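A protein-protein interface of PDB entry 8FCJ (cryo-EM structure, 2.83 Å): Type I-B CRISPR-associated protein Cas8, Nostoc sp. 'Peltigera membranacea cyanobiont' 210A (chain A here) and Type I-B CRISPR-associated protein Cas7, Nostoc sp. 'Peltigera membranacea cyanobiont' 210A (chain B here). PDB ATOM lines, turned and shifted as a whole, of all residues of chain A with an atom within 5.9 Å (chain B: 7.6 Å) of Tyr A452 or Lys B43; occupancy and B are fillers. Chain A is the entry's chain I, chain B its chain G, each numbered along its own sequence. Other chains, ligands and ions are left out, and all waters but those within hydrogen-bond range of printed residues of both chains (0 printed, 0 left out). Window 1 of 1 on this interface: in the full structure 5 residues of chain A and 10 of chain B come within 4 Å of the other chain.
The side-chain hydroxyl of Tyr B151 lies close to the side-chain carboxylate of Glu B174, at 3.1 Å. OD1 of Asp B152 lies within hydrogen-bond range of N of Ala B154 (3.5 Å). N of Tyr A452 sits at hydrogen-bond distance from OG of Ser A456 (3.4 Å). The backbone carbonyl oxygen of Ile B40 lies within hydrogen-bond range of the backbone NH of Asp B32 (2.8 Å). The backbone carbonyl oxygen of Ala B154 lies within hydrogen-bond range of the side-chain hydroxyl of Tyr B151. The backbone carbonyl oxygen (O) of Ile B51 sits at hydrogen-bond distance from the backbone NH (N) of Tyr B151, 2.6 Å away.
Of the printed residues of chain B, Asn A449 touches Arg B35. Printed residues of chain B within 4 Å of Tyr A452: Lys B43 (3.7 Å), Ile B51 (3.5 Å), Tyr B151 (3.6 Å), Asp B152 (3.8 Å) and Gly B153 (3.3 Å). Of the printed residues of chain B, Asp A453 touches Ile B51 (3.8 Å). Arg A494 touches none of the printed residues of chain B. His B31 touches none of the printed residues of chain A. Of the printed residues of chain A, Ile B40 touches Tyr A450 (3.5 Å). Lys B43 touches just one residue of chain A: Tyr A452 (3.7 Å). Of the printed residues of chain A, Asp B152 touches Tyr A452. Printed residues of chain A within 4 Å of Gly B153: Tyr A452 (3.3 Å). The nearest residue of chain B that does not touch Tyr A452 is Glu B174 (4.3 Å). The nearest residue of chain A that does not touch Lys B43 is Tyr A450 (4.9 Å).
Among the printed residues, merely in contact across the chains: Tyr A452 with Gly B153 (3.3 Å), Tyr A450 with Ile B40 (3.5 Å), Tyr A452 with Ile B51 (3.5 Å), Tyr A452 with Tyr B151 (3.6 Å), Tyr A452 with Lys B43 (3.7 Å), Tyr A452 with Asp B152 (3.8 Å), Asp A453 with Ile B51 (3.8 Å) and Asn A449 with Arg B35 (3.9 Å).
Printed residues of chain B that touch a printed residue of chain A: Arg B35, Ile B40, Lys B43, Ile B51, Tyr B151, Asp B152, Gly B153 and Glu B174. Hydrophobic or aromatic side chains of chain B that line the printed part of chain A: Ile B40, Ile B51 and Tyr B151. Hydrophobic or aromatic side chains of chain A that line the printed part of chain B: Tyr A450 and Tyr A452. Among the printed residues, 9 pairs touch across the chains. Among the printed residues, no Asp or Glu carboxylate lies within 4 Å of a Lys or Arg side-chain nitrogen of the other chain.
OE2 of Glu B174 lies within hydrogen-bond range of OH of Tyr A450 (2.7 Å).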
ATOM      1  N   ASN A 449     -19.971   2.733   8.286  1.00  0.00           N
ATOM      2  CA  ASN A 449     -18.585   2.366   8.541  1.00  0.00           C
ATOM      3  C   ASN A 449     -18.367   1.892   9.970  1.00  0.00           C
ATOM      4  O   ASN A 449     -17.425   1.134  10.220  1.00  0.00           O
ATOM      5  CB  ASN A 449     -17.671   3.553   8.246  1.00  0.00           C
ATOM      6  CG  ASN A 449     -16.291   3.131   7.797  1.00  0.00           C
ATOM      7  OD1 ASN A 449     -15.869   1.999   8.029  1.00  0.00           O
ATOM      8  ND2 ASN A 449     -15.576   4.042   7.152  1.00  0.00           N
ATOM      9  N   TYR A 450     -19.211   2.324  10.909  1.00  0.00           N
ATOM     10  CA  TYR A 450     -19.052   1.901  12.296  1.00  0.00           C
ATOM     11  C   TYR A 450     -19.206   0.394  12.441  1.00  0.00           C
ATOM     12  O   TYR A 450     -18.504  -0.234  13.241  1.00  0.00           O
ATOM     13  CB  TYR A 450     -20.055   2.639  13.187  1.00  0.00           C
ATOM     14  CG  TYR A 450     -20.196   2.077  14.590  1.00  0.00           C
ATOM     15  CD1 TYR A 450     -21.021   0.987  14.851  1.00  0.00           C
ATOM     16  CD2 TYR A 450     -19.551   2.672  15.661  1.00  0.00           C
ATOM     17  CE1 TYR A 450     -21.157   0.482  16.127  1.00  0.00           C
ATOM     18  CE2 TYR A 450     -19.685   2.174  16.942  1.00  0.00           C
ATOM     19  CZ  TYR A 450     -20.490   1.081  17.169  1.00  0.00           C
ATOM     20  OH  TYR A 450     -20.628   0.585  18.444  1.00  0.00           O
ATOM     21  N   CYS A 451     -20.128  -0.202  11.688  1.00  0.00           N
ATOM     22  CA  CYS A 451     -20.425  -1.620  11.841  1.00  0.00           C
ATOM     23  C   CYS A 451     -19.191  -2.469  11.567  1.00  0.00           C
ATOM     24  O   CYS A 451     -18.465  -2.247  10.595  1.00  0.00           O
ATOM     25  CB  CYS A 451     -21.559  -2.017  10.900  1.00  0.00           C
ATOM     26  SG  CYS A 451     -22.915  -0.827  10.844  1.00  0.00           S
ATOM     27  N   TYR A 452     -18.957  -3.451  12.438  1.00  0.00           N
ATOM     28  CA  TYR A 452     -17.748  -4.259  12.381  1.00  0.00           C
ATOM     29  C   TYR A 452     -17.992  -5.742  12.143  1.00  0.00           C
ATOM     30  O   TYR A 452     -17.083  -6.418  11.650  1.00  0.00           O
ATOM     31  CB  TYR A 452     -16.936  -4.103  13.675  1.00  0.00           C
ATOM     32  CG  TYR A 452     -17.741  -4.295  14.939  1.00  0.00           C
ATOM     33  CD1 TYR A 452     -17.881  -5.549  15.509  1.00  0.00           C
ATOM     34  CD2 TYR A 452     -18.357  -3.220  15.563  1.00  0.00           C
ATOM     35  CE1 TYR A 452     -18.612  -5.731  16.663  1.00  0.00           C
ATOM     36  CE2 TYR A 452     -19.091  -3.393  16.716  1.00  0.00           C
ATOM     37  CZ  TYR A 452     -19.215  -4.650  17.261  1.00  0.00           C
ATOM     38  OH  TYR A 452     -19.945  -4.831  18.411  1.00  0.00           O
ATOM     39  N   ASP A 453     -19.168  -6.267  12.475  1.00  0.00           N
ATOM     40  CA  ASP A 453     -19.472  -7.672  12.249  1.00  0.00           C
ATOM     41  C   ASP A 453     -20.896  -7.791  11.725  1.00  0.00           C
ATOM     42  O   ASP A 453     -21.600  -6.793  11.543  1.00  0.00           O
ATOM     43  CB  ASP A 453     -19.271  -8.502  13.521  1.00  0.00           C
ATOM     44  CG  ASP A 453     -20.265  -8.156  14.606  1.00  0.00           C
ATOM     45  OD1 ASP A 453     -20.797  -7.027  14.591  1.00  0.00           O
ATOM     46  OD2 ASP A 453     -20.516  -9.014  15.476  1.00  0.00           O
ATOM     47  N   GLU A 454     -21.319  -9.032  11.480  1.00  0.00           N
ATOM     48  CA  GLU A 454     -22.625  -9.270  10.877  1.00  0.00           C
ATOM     49  C   GLU A 454     -23.753  -8.787  11.780  1.00  0.00           C
ATOM     50  O   GLU A 454     -24.693  -8.131  11.318  1.00  0.00           O
ATOM     51  CB  GLU A 454     -22.788 -10.756  10.563  1.00  0.00           C
ATOM     52  CG  GLU A 454     -24.231 -11.211  10.461  1.00  0.00           C
ATOM     53  CD  GLU A 454     -24.382 -12.482   9.655  1.00  0.00           C
ATOM     54  OE1 GLU A 454     -23.390 -12.910   9.028  1.00  0.00           O
ATOM     55  OE2 GLU A 454     -25.493 -13.054   9.645  1.00  0.00           O
ATOM     56  N   SER A 456     -23.912  -6.511  14.299  1.00  0.00           N
ATOM     57  CA  SER A 456     -24.044  -5.066  14.446  1.00  0.00           C
ATOM     58  C   SER A 456     -24.552  -4.420  13.165  1.00  0.00           C
ATOM     59  O   SER A 456     -25.443  -3.562  13.205  1.00  0.00           O
ATOM     60  CB  SER A 456     -22.704  -4.458  14.853  1.00  0.00           C
ATOM     61  OG  SER A 456     -21.722  -4.702  13.863  1.00  0.00           O
ATOM     62  N   PHE A 457     -23.999  -4.819  12.017  1.00  0.00           N
ATOM     63  CA  PHE A 457     -24.425  -4.217  10.761  1.00  0.00           C
ATOM     64  C   PHE A 457     -25.878  -4.537  10.459  1.00  0.00           C
ATOM     65  O   PHE A 457     -26.630  -3.663  10.017  1.00  0.00           O
ATOM     66  CB  PHE A 457     -23.547  -4.683   9.605  1.00  0.00           C
ATOM     67  CG  PHE A 457     -24.070  -4.267   8.264  1.00  0.00           C
ATOM     68  CD1 PHE A 457     -23.908  -2.968   7.818  1.00  0.00           C
ATOM     69  CD2 PHE A 457     -24.752  -5.162   7.462  1.00  0.00           C
ATOM     70  CE1 PHE A 457     -24.398  -2.577   6.592  1.00  0.00           C
ATOM     71  CE2 PHE A 457     -25.246  -4.774   6.237  1.00  0.00           C
ATOM     72  CZ  PHE A 457     -25.067  -3.481   5.801  1.00  0.00           C
ATOM     73  N   TRP A 490     -22.601  -9.659   5.235  1.00  0.00           N
ATOM     74  CA  TRP A 490     -22.901  -8.277   5.592  1.00  0.00           C
ATOM     75  C   TRP A 490     -22.031  -7.288   4.826  1.00  0.00           C
ATOM     76  O   TRP A 490     -22.446  -6.144   4.612  1.00  0.00           O
ATOM     77  CB  TRP A 490     -22.748  -8.080   7.100  1.00  0.00           C
ATOM     78  CG  TRP A 490     -21.338  -8.091   7.584  1.00  0.00           C
ATOM     79  CD1 TRP A 490     -20.586  -9.183   7.890  1.00  0.00           C
ATOM     80  CD2 TRP A 490     -20.512  -6.950   7.836  1.00  0.00           C
ATOM     81  NE1 TRP A 490     -19.339  -8.795   8.310  1.00  0.00           N
ATOM     82  CE2 TRP A 490     -19.268  -7.428   8.286  1.00  0.00           C
ATOM     83  CE3 TRP A 490     -20.701  -5.571   7.719  1.00  0.00           C
ATOM     84  CZ2 TRP A 490     -18.221  -6.578   8.621  1.00  0.00           C
ATOM     85  CZ3 TRP A 490     -19.660  -4.729   8.051  1.00  0.00           C
ATOM     86  CH2 TRP A 490     -18.436  -5.234   8.497  1.00  0.00           C
ATOM     87  N   GLN A 491     -20.833  -7.699   4.406  1.00  0.00           N
ATOM     88  CA  GLN A 491     -19.983  -6.805   3.626  1.00  0.00           C
ATOM     89  C   GLN A 491     -20.613  -6.476   2.279  1.00  0.00           C
ATOM     90  O   GLN A 491     -20.574  -5.323   1.832  1.00  0.00           O
ATOM     91  CB  GLN A 491     -18.605  -7.430   3.431  1.00  0.00           C
ATOM     92  CG  GLN A 491     -18.105  -8.223   4.621  1.00  0.00           C
ATOM     93  CD  GLN A 491     -16.926  -7.560   5.300  1.00  0.00           C
ATOM     94  OE1 GLN A 491     -16.406  -6.556   4.820  1.00  0.00           O
ATOM     95  NE2 GLN A 491     -16.491  -8.127   6.417  1.00  0.00           N
ATOM     96  N   ARG A 494     -23.364  -4.057   2.823  1.00  0.00           N
ATOM     97  CA  ARG A 494     -22.823  -2.721   3.055  1.00  0.00           C
ATOM     98  C   ARG A 494     -22.392  -2.064   1.751  1.00  0.00           C
ATOM     99  O   ARG A 494     -22.633  -0.870   1.538  1.00  0.00           O
ATOM    100  CB  ARG A 494     -21.650  -2.792   4.030  1.00  0.00           C
ATOM    101  CG  ARG A 494     -21.246  -1.449   4.606  1.00  0.00           C
ATOM    102  CD  ARG A 494     -20.324  -1.619   5.796  1.00  0.00           C
ATOM    103  NE  ARG A 494     -19.053  -2.219   5.415  1.00  0.00           N
ATOM    104  CZ  ARG A 494     -17.999  -2.307   6.214  1.00  0.00           C
ATOM    105  NH1 ARG A 494     -18.030  -1.842   7.451  1.00  0.00           N
ATOM    106  NH2 ARG A 494     -16.888  -2.879   5.762  1.00  0.00           N
ATOM    107  N   ASN B  30      -7.096   1.170  22.938  1.00  0.00           N
ATOM    108  CA  ASN B  30      -6.659   0.788  21.601  1.00  0.00           C
ATOM    109  C   ASN B  30      -7.541   1.405  20.528  1.00  0.00           C
ATOM    110  O   ASN B  30      -8.039   0.721  19.634  1.00  0.00           O
ATOM    111  CB  ASN B  30      -6.630  -0.728  21.477  1.00  0.00           C
ATOM    112  CG  ASN B  30      -7.840  -1.388  22.108  1.00  0.00           C
ATOM    113  OD1 ASN B  30      -8.392  -0.891  23.090  1.00  0.00           O
ATOM    114  ND2 ASN B  30      -8.254  -2.520  21.552  1.00  0.00           N
ATOM    115  N   HIS B  31      -7.760   2.712  20.605  1.00  0.00           N
ATOM    116  CA  HIS B  31      -8.521   3.390  19.563  1.00  0.00           C
ATOM    117  C   HIS B  31      -7.801   3.299  18.225  1.00  0.00           C
ATOM    118  O   HIS B  31      -6.569   3.300  18.167  1.00  0.00           O
ATOM    119  CB  HIS B  31      -8.749   4.852  19.939  1.00  0.00           C
ATOM    120  CG  HIS B  31      -9.288   5.041  21.319  1.00  0.00           C
ATOM    121  ND1 HIS B  31     -10.420   4.398  21.767  1.00  0.00           N
ATOM    122  CD2 HIS B  31      -8.853   5.802  22.351  1.00  0.00           C
ATOM    123  CE1 HIS B  31     -10.661   4.755  23.015  1.00  0.00           C
ATOM    124  NE2 HIS B  31      -9.723   5.605  23.394  1.00  0.00           N
ATOM    125  N   ASP B  32      -8.572   3.195  17.151  1.00  0.00           N
ATOM    126  CA  ASP B  32      -8.053   3.290  15.798  1.00  0.00           C
ATOM    127  C   ASP B  32      -8.723   4.466  15.089  1.00  0.00           C
ATOM    128  O   ASP B  32      -9.394   5.290  15.716  1.00  0.00           O
ATOM    129  CB  ASP B  32      -8.235   1.964  15.056  1.00  0.00           C
ATOM    130  CG  ASP B  32      -9.675   1.682  14.693  1.00  0.00           C
ATOM    131  OD1 ASP B  32     -10.577   2.347  15.237  1.00  0.00           O
ATOM    132  OD2 ASP B  32      -9.903   0.788  13.853  1.00  0.00           O
ATOM    133  N   ARG B  35     -14.538   6.645  13.095  1.00  0.00           N
ATOM    134  CA  ARG B  35     -15.563   6.711  12.058  1.00  0.00           C
ATOM    135  C   ARG B  35     -16.560   7.791  12.456  1.00  0.00           C
ATOM    136  O   ARG B  35     -17.501   7.536  13.213  1.00  0.00           O
ATOM    137  CB  ARG B  35     -16.243   5.359  11.875  1.00  0.00           C
ATOM    138  CG  ARG B  35     -15.412   4.183  12.339  1.00  0.00           C
ATOM    139  CD  ARG B  35     -14.460   3.721  11.255  1.00  0.00           C
ATOM    140  NE  ARG B  35     -13.977   2.367  11.496  1.00  0.00           N
ATOM    141  CZ  ARG B  35     -12.956   1.813  10.859  1.00  0.00           C
ATOM    142  NH1 ARG B  35     -12.280   2.472   9.932  1.00  0.00           N
ATOM    143  NH2 ARG B  35     -12.602   0.568  11.162  1.00  0.00           N
ATOM    144  N   THR B  39     -15.708   6.908  18.615  1.00  0.00           N
ATOM    145  CA  THR B  39     -14.312   6.488  18.658  1.00  0.00           C
ATOM    146  C   THR B  39     -14.266   4.966  18.712  1.00  0.00           C
ATOM    147  O   THR B  39     -14.737   4.356  19.676  1.00  0.00           O
ATOM    148  CB  THR B  39     -13.600   7.101  19.859  1.00  0.00           C
ATOM    149  OG1 THR B  39     -13.664   8.529  19.777  1.00  0.00           O
ATOM    150  CG2 THR B  39     -12.149   6.669  19.890  1.00  0.00           C
ATOM    151  N   ILE B  40     -13.694   4.357  17.682  1.00  0.00           N
ATOM    152  CA  ILE B  40     -13.661   2.907  17.549  1.00  0.00           C
ATOM    153  C   ILE B  40     -12.374   2.391  18.171  1.00  0.00           C
ATOM    154  O   ILE B  40     -11.288   2.912  17.893  1.00  0.00           O
ATOM    155  CB  ILE B  40     -13.762   2.494  16.073  1.00  0.00           C
ATOM    156  CG1 ILE B  40     -15.194   2.648  15.572  1.00  0.00           C
ATOM    157  CG2 ILE B  40     -13.332   1.052  15.892  1.00  0.00           C
ATOM    158  CD1 ILE B  40     -16.227   2.249  16.575  1.00  0.00           C
ATOM    159  N   LEU B  41     -12.486   1.375  19.021  1.00  0.00           N
ATOM    160  CA  LEU B  41     -11.304   0.732  19.570  1.00  0.00           C
ATOM    161  C   LEU B  41     -10.913  -0.450  18.693  1.00  0.00           C
ATOM    162  O   LEU B  41     -11.763  -1.097  18.077  1.00  0.00           O
ATOM    163  CB  LEU B  41     -11.540   0.280  21.013  1.00  0.00           C
ATOM    164  CG  LEU B  41     -12.146  -1.093  21.297  1.00  0.00           C
ATOM    165  CD1 LEU B  41     -11.848  -1.503  22.725  1.00  0.00           C
ATOM    166  CD2 LEU B  41     -13.633  -1.095  21.049  1.00  0.00           C
ATOM    167  N   GLN B  42      -9.610  -0.713  18.627  1.00  0.00           N
ATOM    168  CA  GLN B  42      -9.093  -1.725  17.715  1.00  0.00           C
ATOM    169  C   GLN B  42      -9.628  -3.103  18.078  1.00  0.00           C
ATOM    170  O   GLN B  42      -9.582  -3.512  19.240  1.00  0.00           O
ATOM    171  CB  GLN B  42      -7.567  -1.727  17.745  1.00  0.00           C
ATOM    172  CG  GLN B  42      -6.934  -2.903  17.040  1.00  0.00           C
ATOM    173  CD  GLN B  42      -6.413  -2.537  15.670  1.00  0.00           C
ATOM    174  OE1 GLN B  42      -5.878  -1.448  15.471  1.00  0.00           O
ATOM    175  NE2 GLN B  42      -6.572  -3.442  14.714  1.00  0.00           N
ATOM    176  N   LYS B  43     -10.130  -3.819  17.076  1.00  0.00           N
ATOM    177  CA  LYS B  43     -10.715  -5.131  17.302  1.00  0.00           C
ATOM    178  C   LYS B  43     -10.550  -5.977  16.050  1.00  0.00           C
ATOM    179  O   LYS B  43     -10.260  -5.473  14.963  1.00  0.00           O
ATOM    180  CB  LYS B  43     -12.191  -5.029  17.691  1.00  0.00           C
ATOM    181  CG  LYS B  43     -12.955  -3.948  16.956  1.00  0.00           C
ATOM    182  CD  LYS B  43     -14.298  -3.690  17.610  1.00  0.00           C
ATOM    183  CE  LYS B  43     -14.819  -2.310  17.264  1.00  0.00           C
ATOM    184  NZ  LYS B  43     -14.681  -2.025  15.813  1.00  0.00           N
ATOM    185  N   GLY B  44     -10.742  -7.278  16.219  1.00  0.00           N
ATOM    186  CA  GLY B  44     -10.630  -8.208  15.112  1.00  0.00           C
ATOM    187  C   GLY B  44     -11.023  -9.596  15.567  1.00  0.00           C
ATOM    188  O   GLY B  44     -11.356  -9.822  16.734  1.00  0.00           O
ATOM    189  N   TYR B  45     -10.978 -10.529  14.622  1.00  0.00           N
ATOM    190  CA  TYR B  45     -11.401 -11.891  14.900  1.00  0.00           C
ATOM    191  C   TYR B  45     -10.340 -12.647  15.690  1.00  0.00           C
ATOM    192  O   TYR B  45      -9.143 -12.366  15.599  1.00  0.00           O
ATOM    193  CB  TYR B  45     -11.719 -12.626  13.601  1.00  0.00           C
ATOM    194  CG  TYR B  45     -13.022 -12.184  12.985  1.00  0.00           C
ATOM    195  CD1 TYR B  45     -14.230 -12.693  13.434  1.00  0.00           C
ATOM    196  CD2 TYR B  45     -13.046 -11.244  11.966  1.00  0.00           C
ATOM    197  CE1 TYR B  45     -15.424 -12.287  12.881  1.00  0.00           C
ATOM    198  CE2 TYR B  45     -14.235 -10.833  11.407  1.00  0.00           C
ATOM    199  CZ  TYR B  45     -15.421 -11.357  11.868  1.00  0.00           C
ATOM    200  OH  TYR B  45     -16.611 -10.949  11.312  1.00  0.00           O
ATOM    201  N   ILE B  51     -15.411 -11.527  17.734  1.00  0.00           N
ATOM    202  CA  ILE B  51     -14.562 -10.346  17.633  1.00  0.00           C
ATOM    203  C   ILE B  51     -14.032  -9.983  19.013  1.00  0.00           C
ATOM    204  O   ILE B  51     -14.802  -9.818  19.966  1.00  0.00           O
ATOM    205  CB  ILE B  51     -15.332  -9.176  17.005  1.00  0.00           C
ATOM    206  CG1 ILE B  51     -15.566  -9.444  15.517  1.00  0.00           C
ATOM    207  CG2 ILE B  51     -14.584  -7.872  17.218  1.00  0.00           C
ATOM    208  CD1 ILE B  51     -15.681  -8.200  14.673  1.00  0.00           C
ATOM    209  N   HIS B  52     -12.714  -9.856  19.117  1.00  0.00           N
ATOM    210  CA  HIS B  52     -12.046  -9.464  20.347  1.00  0.00           C
ATOM    211  C   HIS B  52     -11.335  -8.138  20.129  1.00  0.00           C
ATOM    212  O   HIS B  52     -10.996  -7.781  19.000  1.00  0.00           O
ATOM    213  CB  HIS B  52     -11.034 -10.521  20.793  1.00  0.00           C
ATOM    214  CG  HIS B  52     -11.657 -11.799  21.258  1.00  0.00           C
ATOM    215  ND1 HIS B  52     -11.376 -12.359  22.483  1.00  0.00           N
ATOM    216  CD2 HIS B  52     -12.543 -12.626  20.658  1.00  0.00           C
ATOM    217  CE1 HIS B  52     -12.064 -13.478  22.620  1.00  0.00           C
ATOM    218  NE2 HIS B  52     -12.781 -13.662  21.528  1.00  0.00           N
ATOM    219  N   SER B  53     -11.108  -7.413  21.218  1.00  0.00           N
ATOM    220  CA  SER B  53     -10.393  -6.146  21.158  1.00  0.00           C
ATOM    221  C   SER B  53      -8.917  -6.385  21.440  1.00  0.00           C
ATOM    222  O   SER B  53      -8.565  -7.046  22.420  1.00  0.00           O
ATOM    223  CB  SER B  53     -10.974  -5.148  22.157  1.00  0.00           C
ATOM    224  OG  SER B  53     -10.642  -5.506  23.485  1.00  0.00           O
ATOM    225  N   PHE B  54      -8.060  -5.850  20.577  1.00  0.00           N
ATOM    226  CA  PHE B  54      -6.621  -6.033  20.677  1.00  0.00           C
ATOM    227  C   PHE B  54      -5.961  -4.750  21.157  1.00  0.00           C
ATOM    228  O   PHE B  54      -6.336  -3.656  20.732  1.00  0.00           O
ATOM    229  CB  PHE B  54      -6.015  -6.426  19.329  1.00  0.00           C
ATOM    230  CG  PHE B  54      -6.611  -7.659  18.730  1.00  0.00           C
ATOM    231  CD1 PHE B  54      -6.567  -8.862  19.404  1.00  0.00           C
ATOM    232  CD2 PHE B  54      -7.202  -7.619  17.484  1.00  0.00           C
ATOM    233  CE1 PHE B  54      -7.110  -9.999  18.851  1.00  0.00           C
ATOM    234  CE2 PHE B  54      -7.745  -8.754  16.927  1.00  0.00           C
ATOM    235  CZ  PHE B  54      -7.698  -9.945  17.612  1.00  0.00           C
ATOM    236  N   VAL B  55      -4.971  -4.891  22.032  1.00  0.00           N
ATOM    237  CA  VAL B  55      -4.115  -3.788  22.450  1.00  0.00           C
ATOM    238  C   VAL B  55      -2.743  -4.012  21.835  1.00  0.00           C
ATOM    239  O   VAL B  55      -2.116  -5.052  22.069  1.00  0.00           O
ATOM    240  CB  VAL B  55      -4.023  -3.686  23.981  1.00  0.00           C
ATOM    241  CG1 VAL B  55      -2.900  -2.752  24.382  1.00  0.00           C
ATOM    242  CG2 VAL B  55      -5.339  -3.213  24.552  1.00  0.00           C
ATOM    243  N   SER B 147      -7.985  -9.361  24.216  1.00  0.00           N
ATOM    244  CA  SER B 147      -9.005  -9.455  25.248  1.00  0.00           C
ATOM    245  C   SER B 147      -9.410 -10.908  25.450  1.00  0.00           C
ATOM    246  O   SER B 147      -9.638 -11.641  24.485  1.00  0.00           O
ATOM    247  CB  SER B 147     -10.222  -8.615  24.871  1.00  0.00           C
ATOM    248  OG  SER B 147     -10.918  -9.193  23.784  1.00  0.00           O
ATOM    249  N   TYR B 151     -15.687  -9.131  22.359  1.00  0.00           N
ATOM    250  CA  TYR B 151     -16.225  -7.782  22.481  1.00  0.00           C
ATOM    251  C   TYR B 151     -17.728  -7.793  22.234  1.00  0.00           C
ATOM    252  O   TYR B 151     -18.185  -8.193  21.159  1.00  0.00           O
ATOM    253  CB  TYR B 151     -15.522  -6.851  21.498  1.00  0.00           C
ATOM    254  CG  TYR B 151     -16.094  -5.458  21.464  1.00  0.00           C
ATOM    255  CD1 TYR B 151     -16.151  -4.685  22.611  1.00  0.00           C
ATOM    256  CD2 TYR B 151     -16.571  -4.913  20.283  1.00  0.00           C
ATOM    257  CE1 TYR B 151     -16.670  -3.412  22.586  1.00  0.00           C
ATOM    258  CE2 TYR B 151     -17.093  -3.640  20.248  1.00  0.00           C
ATOM    259  CZ  TYR B 151     -17.138  -2.895  21.402  1.00  0.00           C
ATOM    260  OH  TYR B 151     -17.659  -1.624  21.377  1.00  0.00           O
ATOM    261  N   ASP B 152     -18.497  -7.351  23.231  1.00  0.00           N
ATOM    262  CA  ASP B 152     -19.951  -7.382  23.125  1.00  0.00           C
ATOM    263  C   ASP B 152     -20.482  -6.269  22.231  1.00  0.00           C
ATOM    264  O   ASP B 152     -21.431  -6.483  21.469  1.00  0.00           O
ATOM    265  CB  ASP B 152     -20.578  -7.285  24.515  1.00  0.00           C
ATOM    266  CG  ASP B 152     -19.737  -6.474  25.474  1.00  0.00           C
ATOM    267  OD1 ASP B 152     -18.931  -5.647  25.001  1.00  0.00           O
ATOM    268  OD2 ASP B 152     -19.879  -6.663  26.699  1.00  0.00           O
ATOM    269  N   GLY B 153     -19.893  -5.081  22.311  1.00  0.00           N
ATOM    270  CA  GLY B 153     -20.368  -3.955  21.534  1.00  0.00           C
ATOM    271  C   GLY B 153     -20.768  -2.781  22.399  1.00  0.00           C
ATOM    272  O   GLY B 153     -21.561  -1.931  21.981  1.00  0.00           O
ATOM    273  N   ALA B 154     -20.224  -2.724  23.610  1.00  0.00           N
ATOM    274  CA  ALA B 154     -20.567  -1.659  24.539  1.00  0.00           C
ATOM    275  C   ALA B 154     -20.021  -0.323  24.056  1.00  0.00           C
ATOM    276  O   ALA B 154     -18.898  -0.236  23.556  1.00  0.00           O
ATOM    277  CB  ALA B 154     -20.023  -1.974  25.930  1.00  0.00           C
ATOM    278  N   GLU B 174     -16.107   3.752  22.594  1.00  0.00           N
ATOM    279  CA  GLU B 174     -16.295   2.328  22.819  1.00  0.00           C
ATOM    280  C   GLU B 174     -15.368   1.855  23.930  1.00  0.00           C
ATOM    281  O   GLU B 174     -14.184   2.205  23.950  1.00  0.00           O
ATOM    282  CB  GLU B 174     -16.028   1.539  21.539  1.00  0.00           C
ATOM    283  CG  GLU B 174     -17.194   1.513  20.577  1.00  0.00           C
ATOM    284  CD  GLU B 174     -16.963   0.571  19.417  1.00  0.00           C
ATOM    285  OE1 GLU B 174     -15.791   0.260  19.127  1.00  0.00           O
ATOM    286  OE2 GLU B 174     -17.954   0.137  18.794  1.00  0.00           O
ATOM    287  N   HIS B 176     -14.504  -1.716  26.670  1.00  0.00           N
ATOM    288  CA  HIS B 176     -14.609  -3.162  26.790  1.00  0.00           C
ATOM    289  C   HIS B 176     -14.302  -3.569  28.221  1.00  0.00           C
ATOM    290  O   HIS B 176     -13.265  -3.187  28.768  1.00  0.00           O
ATOM    291  CB  HIS B 176     -13.654  -3.863  25.822  1.00  0.00           C
ATOM    292  CG  HIS B 176     -13.956  -5.313  25.621  1.00  0.00           C
ATOM    293  ND1 HIS B 176     -13.170  -6.135  24.846  1.00  0.00           N
ATOM    294  CD2 HIS B 176     -14.957  -6.088  26.099  1.00  0.00           C
ATOM    295  CE1 HIS B 176     -13.674  -7.355  24.853  1.00  0.00           C
ATOM    296  NE2 HIS B 176     -14.759  -7.353  25.606  1.00  0.00           N
